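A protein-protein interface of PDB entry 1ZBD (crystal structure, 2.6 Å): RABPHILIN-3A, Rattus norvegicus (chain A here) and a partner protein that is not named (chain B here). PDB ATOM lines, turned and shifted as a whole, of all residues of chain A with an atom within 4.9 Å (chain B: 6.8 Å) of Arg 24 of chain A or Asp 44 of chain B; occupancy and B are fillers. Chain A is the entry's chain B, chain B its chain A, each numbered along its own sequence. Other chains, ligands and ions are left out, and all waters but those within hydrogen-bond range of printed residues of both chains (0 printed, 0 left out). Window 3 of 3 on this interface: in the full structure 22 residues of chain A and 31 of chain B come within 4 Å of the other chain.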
ATOM      1  N   ARG A  20       6.090   7.825  -8.960  1.00  0.00           N
ATOM      2  CA  ARG A  20       6.552   9.014  -9.670  1.00  0.00           C
ATOM      3  C   ARG A  20       6.303   8.812 -11.159  1.00  0.00           C
ATOM      4  O   ARG A  20       5.637   9.622 -11.807  1.00  0.00           O
ATOM      5  CB  ARG A  20       8.048   9.252  -9.452  1.00  0.00           C
ATOM      6  CG  ARG A  20       8.448   9.653  -8.046  1.00  0.00           C
ATOM      7  CD  ARG A  20       9.870  10.203  -8.045  1.00  0.00           C
ATOM      8  NE  ARG A  20      10.351  10.485  -6.698  1.00  0.00           N
ATOM      9  CZ  ARG A  20      10.637   9.553  -5.796  1.00  0.00           C
ATOM     10  NH1 ARG A  20      10.495   8.268  -6.099  1.00  0.00           N
ATOM     11  NH2 ARG A  20      11.065   9.903  -4.591  1.00  0.00           N
ATOM     12  N   VAL A  21       6.852   7.724 -11.693  1.00  0.00           N
ATOM     13  CA  VAL A  21       6.696   7.389 -13.102  1.00  0.00           C
ATOM     14  C   VAL A  21       5.209   7.385 -13.447  1.00  0.00           C
ATOM     15  O   VAL A  21       4.792   7.967 -14.448  1.00  0.00           O
ATOM     16  CB  VAL A  21       7.307   5.997 -13.410  1.00  0.00           C
ATOM     17  CG1 VAL A  21       6.999   5.588 -14.848  1.00  0.00           C
ATOM     18  CG2 VAL A  21       8.815   6.034 -13.188  1.00  0.00           C
ATOM     19  N   ILE A  22       4.414   6.735 -12.604  1.00  0.00           N
ATOM     20  CA  ILE A  22       2.975   6.667 -12.816  1.00  0.00           C
ATOM     21  C   ILE A  22       2.392   8.072 -12.905  1.00  0.00           C
ATOM     22  O   ILE A  22       1.673   8.405 -13.848  1.00  0.00           O
ATOM     23  CB  ILE A  22       2.279   5.920 -11.664  1.00  0.00           C
ATOM     24  CG1 ILE A  22       2.775   4.473 -11.610  1.00  0.00           C
ATOM     25  CG2 ILE A  22       0.770   5.973 -11.848  1.00  0.00           C
ATOM     26  CD1 ILE A  22       2.074   3.612 -10.573  1.00  0.00           C
ATOM     27  N   ALA A  23       2.722   8.892 -11.916  1.00  0.00           N
ATOM     28  CA  ALA A  23       2.247  10.267 -11.841  1.00  0.00           C
ATOM     29  C   ALA A  23       2.499  11.058 -13.114  1.00  0.00           C
ATOM     30  O   ALA A  23       1.597  11.727 -13.619  1.00  0.00           O
ATOM     31  CB  ALA A  23       2.903  10.976 -10.660  1.00  0.00           C
ATOM     32  N   ARG A  24       3.724  10.993 -13.631  1.00  0.00           N
ATOM     33  CA  ARG A  24       4.056  11.739 -14.834  1.00  0.00           C
ATOM     34  C   ARG A  24       3.567  11.050 -16.097  1.00  0.00           C
ATOM     35  O   ARG A  24       3.685  11.592 -17.197  1.00  0.00           O
ATOM     36  CB  ARG A  24       5.566  12.016 -14.909  1.00  0.00           C
ATOM     37  CG  ARG A  24       6.470  10.812 -15.066  1.00  0.00           C
ATOM     38  CD  ARG A  24       7.931  11.239 -14.899  1.00  0.00           C
ATOM     39  NE  ARG A  24       8.861  10.124 -15.059  1.00  0.00           N
ATOM     40  CZ  ARG A  24       9.409   9.753 -16.215  1.00  0.00           C
ATOM     41  NH1 ARG A  24       9.127  10.410 -17.332  1.00  0.00           N
ATOM     42  NH2 ARG A  24      10.247   8.723 -16.251  1.00  0.00           N
ATOM     43  N   ALA A  25       3.008   9.857 -15.935  1.00  0.00           N
ATOM     44  CA  ALA A  25       2.479   9.121 -17.070  1.00  0.00           C
ATOM     45  C   ALA A  25       1.010   9.491 -17.158  1.00  0.00           C
ATOM     46  O   ALA A  25       0.455   9.644 -18.251  1.00  0.00           O
ATOM     47  CB  ALA A  25       2.636   7.623 -16.856  1.00  0.00           C
ATOM     48  N   GLU A  26       0.388   9.640 -15.990  1.00  0.00           N
ATOM     49  CA  GLU A  26      -1.023  10.003 -15.903  1.00  0.00           C
ATOM     50  C   GLU A  26      -1.223  11.446 -16.335  1.00  0.00           C
ATOM     51  O   GLU A  26      -2.295  11.820 -16.810  1.00  0.00           O
ATOM     52  CB  GLU A  26      -1.544   9.807 -14.474  1.00  0.00           C
ATOM     53  CG  GLU A  26      -1.733   8.340 -14.082  1.00  0.00           C
ATOM     54  CD  GLU A  26      -2.298   8.161 -12.678  1.00  0.00           C
ATOM     55  OE1 GLU A  26      -2.431   9.170 -11.949  1.00  0.00           O
ATOM     56  OE2 GLU A  26      -2.606   7.007 -12.302  1.00  0.00           O
ATOM     57  N   LYS A  27      -0.183  12.255 -16.174  1.00  0.00           N
ATOM     58  CA  LYS A  27      -0.257  13.652 -16.567  1.00  0.00           C
ATOM     59  C   LYS A  27      -0.198  13.716 -18.090  1.00  0.00           C
ATOM     60  O   LYS A  27      -0.806  14.582 -18.718  1.00  0.00           O
ATOM     61  CB  LYS A  27       0.905  14.443 -15.958  1.00  0.00           C
ATOM     62  CG  LYS A  27       0.843  15.931 -16.246  1.00  0.00           C
ATOM     63  CD  LYS A  27       1.889  16.718 -15.472  1.00  0.00           C
ATOM     64  CE  LYS A  27       1.662  18.219 -15.645  1.00  0.00           C
ATOM     65  NZ  LYS A  27       2.621  19.047 -14.864  1.00  0.00           N
ATOM     66  N   MET A  28       0.541  12.780 -18.674  1.00  0.00           N
ATOM     67  CA  MET A  28       0.686  12.714 -20.119  1.00  0.00           C
ATOM     68  C   MET A  28      -0.624  12.203 -20.703  1.00  0.00           C
ATOM     69  O   MET A  28      -1.008  12.573 -21.812  1.00  0.00           O
ATOM     70  CB  MET A  28       1.847  11.775 -20.481  1.00  0.00           C
ATOM     71  CG  MET A  28       2.270  11.802 -21.942  1.00  0.00           C
ATOM     72  SD  MET A  28       4.002  11.287 -22.164  1.00  0.00           S
ATOM     73  CE  MET A  28       4.788  12.874 -22.519  1.00  0.00           C
ATOM     74  N   LEU B  25      17.639   1.632 -24.589  1.00  0.00           N
ATOM     75  CA  LEU B  25      16.844   2.848 -24.530  1.00  0.00           C
ATOM     76  C   LEU B  25      17.735   4.092 -24.430  1.00  0.00           C
ATOM     77  O   LEU B  25      17.700   4.960 -25.308  1.00  0.00           O
ATOM     78  CB  LEU B  25      15.883   2.791 -23.336  1.00  0.00           C
ATOM     79  CG  LEU B  25      14.953   3.995 -23.225  1.00  0.00           C
ATOM     80  CD1 LEU B  25      14.196   4.157 -24.525  1.00  0.00           C
ATOM     81  CD2 LEU B  25      13.996   3.819 -22.061  1.00  0.00           C
ATOM     82  N   PHE B  26      18.533   4.174 -23.366  1.00  0.00           N
ATOM     83  CA  PHE B  26      19.426   5.315 -23.166  1.00  0.00           C
ATOM     84  C   PHE B  26      20.277   5.628 -24.390  1.00  0.00           C
ATOM     85  O   PHE B  26      20.691   6.768 -24.580  1.00  0.00           O
ATOM     86  CB  PHE B  26      20.341   5.088 -21.962  1.00  0.00           C
ATOM     87  CG  PHE B  26      19.738   5.512 -20.650  1.00  0.00           C
ATOM     88  CD1 PHE B  26      19.304   6.821 -20.460  1.00  0.00           C
ATOM     89  CD2 PHE B  26      19.622   4.611 -19.596  1.00  0.00           C
ATOM     90  CE1 PHE B  26      18.763   7.227 -19.237  1.00  0.00           C
ATOM     91  CE2 PHE B  26      19.081   5.007 -18.369  1.00  0.00           C
ATOM     92  CZ  PHE B  26      18.651   6.316 -18.190  1.00  0.00           C
ATOM     93  N   THR B  40      16.392  -2.102 -13.110  1.00  0.00           N
ATOM     94  CA  THR B  40      15.247  -1.201 -13.126  1.00  0.00           C
ATOM     95  C   THR B  40      14.188  -1.583 -12.092  1.00  0.00           C
ATOM     96  O   THR B  40      13.871  -2.761 -11.907  1.00  0.00           O
ATOM     97  CB  THR B  40      14.600  -1.187 -14.523  1.00  0.00           C
ATOM     98  OG1 THR B  40      15.570  -0.768 -15.491  1.00  0.00           O
ATOM     99  CG2 THR B  40      13.406  -0.244 -14.556  1.00  0.00           C
ATOM    100  N   VAL B  41      13.636  -0.576 -11.422  1.00  0.00           N
ATOM    101  CA  VAL B  41      12.615  -0.813 -10.410  1.00  0.00           C
ATOM    102  C   VAL B  41      11.210  -0.713 -11.002  1.00  0.00           C
ATOM    103  O   VAL B  41      10.654   0.377 -11.133  1.00  0.00           O
ATOM    104  CB  VAL B  41      12.744   0.195  -9.245  1.00  0.00           C
ATOM    105  CG1 VAL B  41      11.704  -0.105  -8.173  1.00  0.00           C
ATOM    106  CG2 VAL B  41      14.146   0.130  -8.664  1.00  0.00           C
ATOM    107  N   GLY B  42      10.640  -1.861 -11.355  1.00  0.00           N
ATOM    108  CA  GLY B  42       9.308  -1.877 -11.928  1.00  0.00           C
ATOM    109  C   GLY B  42       9.308  -1.426 -13.375  1.00  0.00           C
ATOM    110  O   GLY B  42       9.577  -2.217 -14.276  1.00  0.00           O
ATOM    111  N   ILE B  43       9.002  -0.152 -13.598  1.00  0.00           N
ATOM    112  CA  ILE B  43       8.969   0.409 -14.944  1.00  0.00           C
ATOM    113  C   ILE B  43       9.467   1.842 -14.972  1.00  0.00           C
ATOM    114  O   ILE B  43       9.663   2.470 -13.929  1.00  0.00           O
ATOM    115  CB  ILE B  43       7.536   0.401 -15.533  1.00  0.00           C
ATOM    116  CG1 ILE B  43       6.518   0.767 -14.449  1.00  0.00           C
ATOM    117  CG2 ILE B  43       7.224  -0.949 -16.138  1.00  0.00           C
ATOM    118  CD1 ILE B  43       6.671   2.166 -13.889  1.00  0.00           C
ATOM    119  N   ASP B  44       9.664   2.349 -16.182  1.00  0.00           N
ATOM    120  CA  ASP B  44      10.106   3.718 -16.398  1.00  0.00           C
ATOM    121  C   ASP B  44       9.940   3.980 -17.880  1.00  0.00           C
ATOM    122  O   ASP B  44       9.821   3.039 -18.657  1.00  0.00           O
ATOM    123  CB  ASP B  44      11.569   3.889 -15.996  1.00  0.00           C
ATOM    124  CG  ASP B  44      12.009   5.342 -16.010  1.00  0.00           C
ATOM    125  OD1 ASP B  44      11.317   6.182 -15.390  1.00  0.00           O
ATOM    126  OD2 ASP B  44      13.048   5.642 -16.634  1.00  0.00           O
ATOM    127  N   PHE B  45       9.922   5.247 -18.282  1.00  0.00           N
ATOM    128  CA  PHE B  45       9.760   5.548 -19.696  1.00  0.00           C
ATOM    129  C   PHE B  45      10.393   6.861 -20.131  1.00  0.00           C
ATOM    130  O   PHE B  45      10.765   7.697 -19.313  1.00  0.00           O
ATOM    131  CB  PHE B  45       8.270   5.538 -20.066  1.00  0.00           C
ATOM    132  CG  PHE B  45       7.481   6.682 -19.482  1.00  0.00           C
ATOM    133  CD1 PHE B  45       7.391   7.900 -20.153  1.00  0.00           C
ATOM    134  CD2 PHE B  45       6.820   6.539 -18.268  1.00  0.00           C
ATOM    135  CE1 PHE B  45       6.647   8.957 -19.624  1.00  0.00           C
ATOM    136  CE2 PHE B  45       6.076   7.590 -17.731  1.00  0.00           C
ATOM    137  CZ  PHE B  45       5.989   8.800 -18.411  1.00  0.00           C
ATOM    138  N   LYS B  46      10.515   7.017 -21.442  1.00  0.00           N
ATOM    139  CA  LYS B  46      11.085   8.209 -22.033  1.00  0.00           C
ATOM    140  C   LYS B  46      10.256   8.564 -23.248  1.00  0.00           C
ATOM    141  O   LYS B  46       9.598   7.702 -23.835  1.00  0.00           O
ATOM    142  CB  LYS B  46      12.533   7.966 -22.464  1.00  0.00           C
ATOM    143  CG  LYS B  46      13.533   8.016 -21.331  1.00  0.00           C
ATOM    144  CD  LYS B  46      14.954   7.809 -21.841  1.00  0.00           C
ATOM    145  CE  LYS B  46      15.982   8.424 -20.892  1.00  0.00           C
ATOM    146  NZ  LYS B  46      15.824   7.968 -19.480  1.00  0.00           N
ATOM    147  N   VAL B  47      10.296   9.839 -23.618  1.00  0.00           N
ATOM    148  CA  VAL B  47       9.562  10.334 -24.767  1.00  0.00           C
ATOM    149  C   VAL B  47      10.523  10.877 -25.808  1.00  0.00           C
ATOM    150  O   VAL B  47      11.507  11.536 -25.480  1.00  0.00           O
ATOM    151  CB  VAL B  47       8.596  11.439 -24.364  1.00  0.00           C
ATOM    152  CG1 VAL B  47       7.998  12.059 -25.597  1.00  0.00           C
ATOM    153  CG2 VAL B  47       7.501  10.863 -23.463  1.00  0.00           C
ATOM    154  N   GLN B  60       6.454   7.020 -26.991  1.00  0.00           N
ATOM    155  CA  GLN B  60       6.532   6.911 -25.542  1.00  0.00           C
ATOM    156  C   GLN B  60       7.119   5.515 -25.338  1.00  0.00           C
ATOM    157  O   GLN B  60       6.413   4.513 -25.428  1.00  0.00           O
ATOM    158  CB  GLN B  60       5.147   7.027 -24.906  1.00  0.00           C
ATOM    159  CG  GLN B  60       5.191   6.963 -23.386  1.00  0.00           C
ATOM    160  CD  GLN B  60       3.832   7.146 -22.737  1.00  0.00           C
ATOM    161  OE1 GLN B  60       2.894   6.386 -22.991  1.00  0.00           O
ATOM    162  NE2 GLN B  60       3.722   8.158 -21.881  1.00  0.00           N
ATOM    163  N   ILE B  61       8.423   5.451 -25.088  1.00  0.00           N
ATOM    164  CA  ILE B  61       9.109   4.173 -24.934  1.00  0.00           C
ATOM    165  C   ILE B  61       9.299   3.734 -23.497  1.00  0.00           C
ATOM    166  O   ILE B  61      10.063   4.351 -22.759  1.00  0.00           O
ATOM    167  CB  ILE B  61      10.486   4.228 -25.606  1.00  0.00           C
ATOM    168  CG1 ILE B  61      10.325   4.696 -27.054  1.00  0.00           C
ATOM    169  CG2 ILE B  61      11.148   2.867 -25.554  1.00  0.00           C
ATOM    170  CD1 ILE B  61      11.632   4.922 -27.780  1.00  0.00           C
ATOM    171  N   TRP B  62       8.615   2.653 -23.115  1.00  0.00           N
ATOM    172  CA  TRP B  62       8.694   2.113 -21.756  1.00  0.00           C
ATOM    173  C   TRP B  62       9.779   1.055 -21.599  1.00  0.00           C
ATOM    174  O   TRP B  62       9.961   0.198 -22.455  1.00  0.00           O
ATOM    175  CB  TRP B  62       7.345   1.504 -21.330  1.00  0.00           C
ATOM    176  CG  TRP B  62       6.202   2.478 -21.325  1.00  0.00           C
ATOM    177  CD1 TRP B  62       5.599   3.041 -22.411  1.00  0.00           C
ATOM    178  CD2 TRP B  62       5.552   3.036 -20.175  1.00  0.00           C
ATOM    179  NE1 TRP B  62       4.614   3.916 -22.011  1.00  0.00           N
ATOM    180  CE2 TRP B  62       4.565   3.929 -20.642  1.00  0.00           C
ATOM    181  CE3 TRP B  62       5.712   2.867 -18.794  1.00  0.00           C
ATOM    182  CZ2 TRP B  62       3.742   4.652 -19.779  1.00  0.00           C
ATOM    183  CZ3 TRP B  62       4.893   3.587 -17.933  1.00  0.00           C
ATOM    184  CH2 TRP B  62       3.920   4.467 -18.430  1.00  0.00           C
ATOM    185  N   ASP B  63      10.485   1.131 -20.481  1.00  0.00           N
ATOM    186  CA  ASP B  63      11.555   0.208 -20.145  1.00  0.00           C
ATOM    187  C   ASP B  63      11.049  -0.597 -18.953  1.00  0.00           C
ATOM    188  O   ASP B  63      10.824  -0.048 -17.877  1.00  0.00           O
ATOM    189  CB  ASP B  63      12.807   1.009 -19.777  1.00  0.00           C
ATOM    190  CG  ASP B  63      13.944   0.140 -19.290  1.00  0.00           C
ATOM    191  OD1 ASP B  63      14.294  -0.842 -19.979  1.00  0.00           O
ATOM    192  OD2 ASP B  63      14.498   0.451 -18.214  1.00  0.00           O
ATOM    193  N   THR B  64      10.861  -1.897 -19.151  1.00  0.00           N
ATOM    194  CA  THR B  64      10.344  -2.757 -18.090  1.00  0.00           C
ATOM    195  C   THR B  64      11.406  -3.551 -17.341  1.00  0.00           C
ATOM    196  O   THR B  64      12.491  -3.815 -17.863  1.00  0.00           O
ATOM    197  CB  THR B  64       9.331  -3.758 -18.655  1.00  0.00           C
ATOM    198  OG1 THR B  64       9.978  -4.590 -19.626  1.00  0.00           O
ATOM    199  CG2 THR B  64       8.180  -3.032 -19.316  1.00  0.00           C
ATOM    200  N   ALA B  65      11.078  -3.937 -16.112  1.00  0.00           N
ATOM    201  CA  ALA B  65      11.988  -4.720 -15.284  1.00  0.00           C
ATOM    202  C   ALA B  65      11.892  -6.168 -15.735  1.00  0.00           C
ATOM    203  O   ALA B  65      10.798  -6.696 -15.899  1.00  0.00           O
ATOM    204  CB  ALA B  65      11.601  -4.606 -13.818  1.00  0.00           C
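Arg 24 of chain A touches two residues of chain B. Printed residues of chain A within 4 Å of Ile 43 of chain B: Val 21. Asp 44 of chain B touches just these residues of chain A: Val 21 and Arg 24. Of the printed residues of chain A, Phe 45 of chain B touches Val 21, Arg 24 and Ala 25. Of the printed residues of chain A, Val 47 of chain B touches Met 28. Printed residues of chain A within 4 Å of Gln 60 of chain B: Met 28. Of the printed residues of chain A, Trp 62 of chain B touches Ala 25 (3.8 Å). The nearest residue of chain B that does not touch Arg 24 of chain A is Lys 46 of chain B (5.5 Å). The nearest printed residue of chain A that does not touch Asp 44 of chain B is Arg 20 of chain A (7.1 Å). The nearest printed residue of chain A that does not touch Trp 62 of chain B is Val 21 of chain A (4.2 Å).
Hydrophobic or aromatic side chains of chain A within 4 Å of the printed part of chain B: Val 21, Ala 25 and Met 28.
Among the printed residues, pairs that only touch across the chains: Val 21 of chain A with Ile 43 of chain B, Val 21 of chain A with Asp 44 of chain B, Val 21 of chain A with Phe 45 of chain B, Ala 25 of chain A with Phe 45 of chain B, Ala 25 of chain A with Trp 62 of chain B and Met 28 of chain A with Val 47 of chain B.
The backbone carbonyl oxygen of Asp 44 of chain B lies within hydrogen-bond range of the backbone NH of Asp 63 of chain B, at 2.7 Å. The side-chain amide oxygen (OE1) of Gln 60 of chain B sits at hydrogen-bond distance from the indole nitrogen (NE1) of Trp 62 of chain B, at 3.2 Å.
The side-chain carboxylate (OD1) of Asp 44 of chain B is in salt-bridge range of the guanidinium group (NH2) of Arg 24 of chain A, 2.9 Å away. The side-chain sulfur (SD) of Met 28 of chain A sits at hydrogen-bond distance from the side-chain amide nitrogen (NE2) of Gln 60 of chain B, 3.2 Å away. The backbone carbonyl oxygen of Phe 45 of chain B sits at hydrogen-bond distance from the guanidinium group of Arg 24 of chain A.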
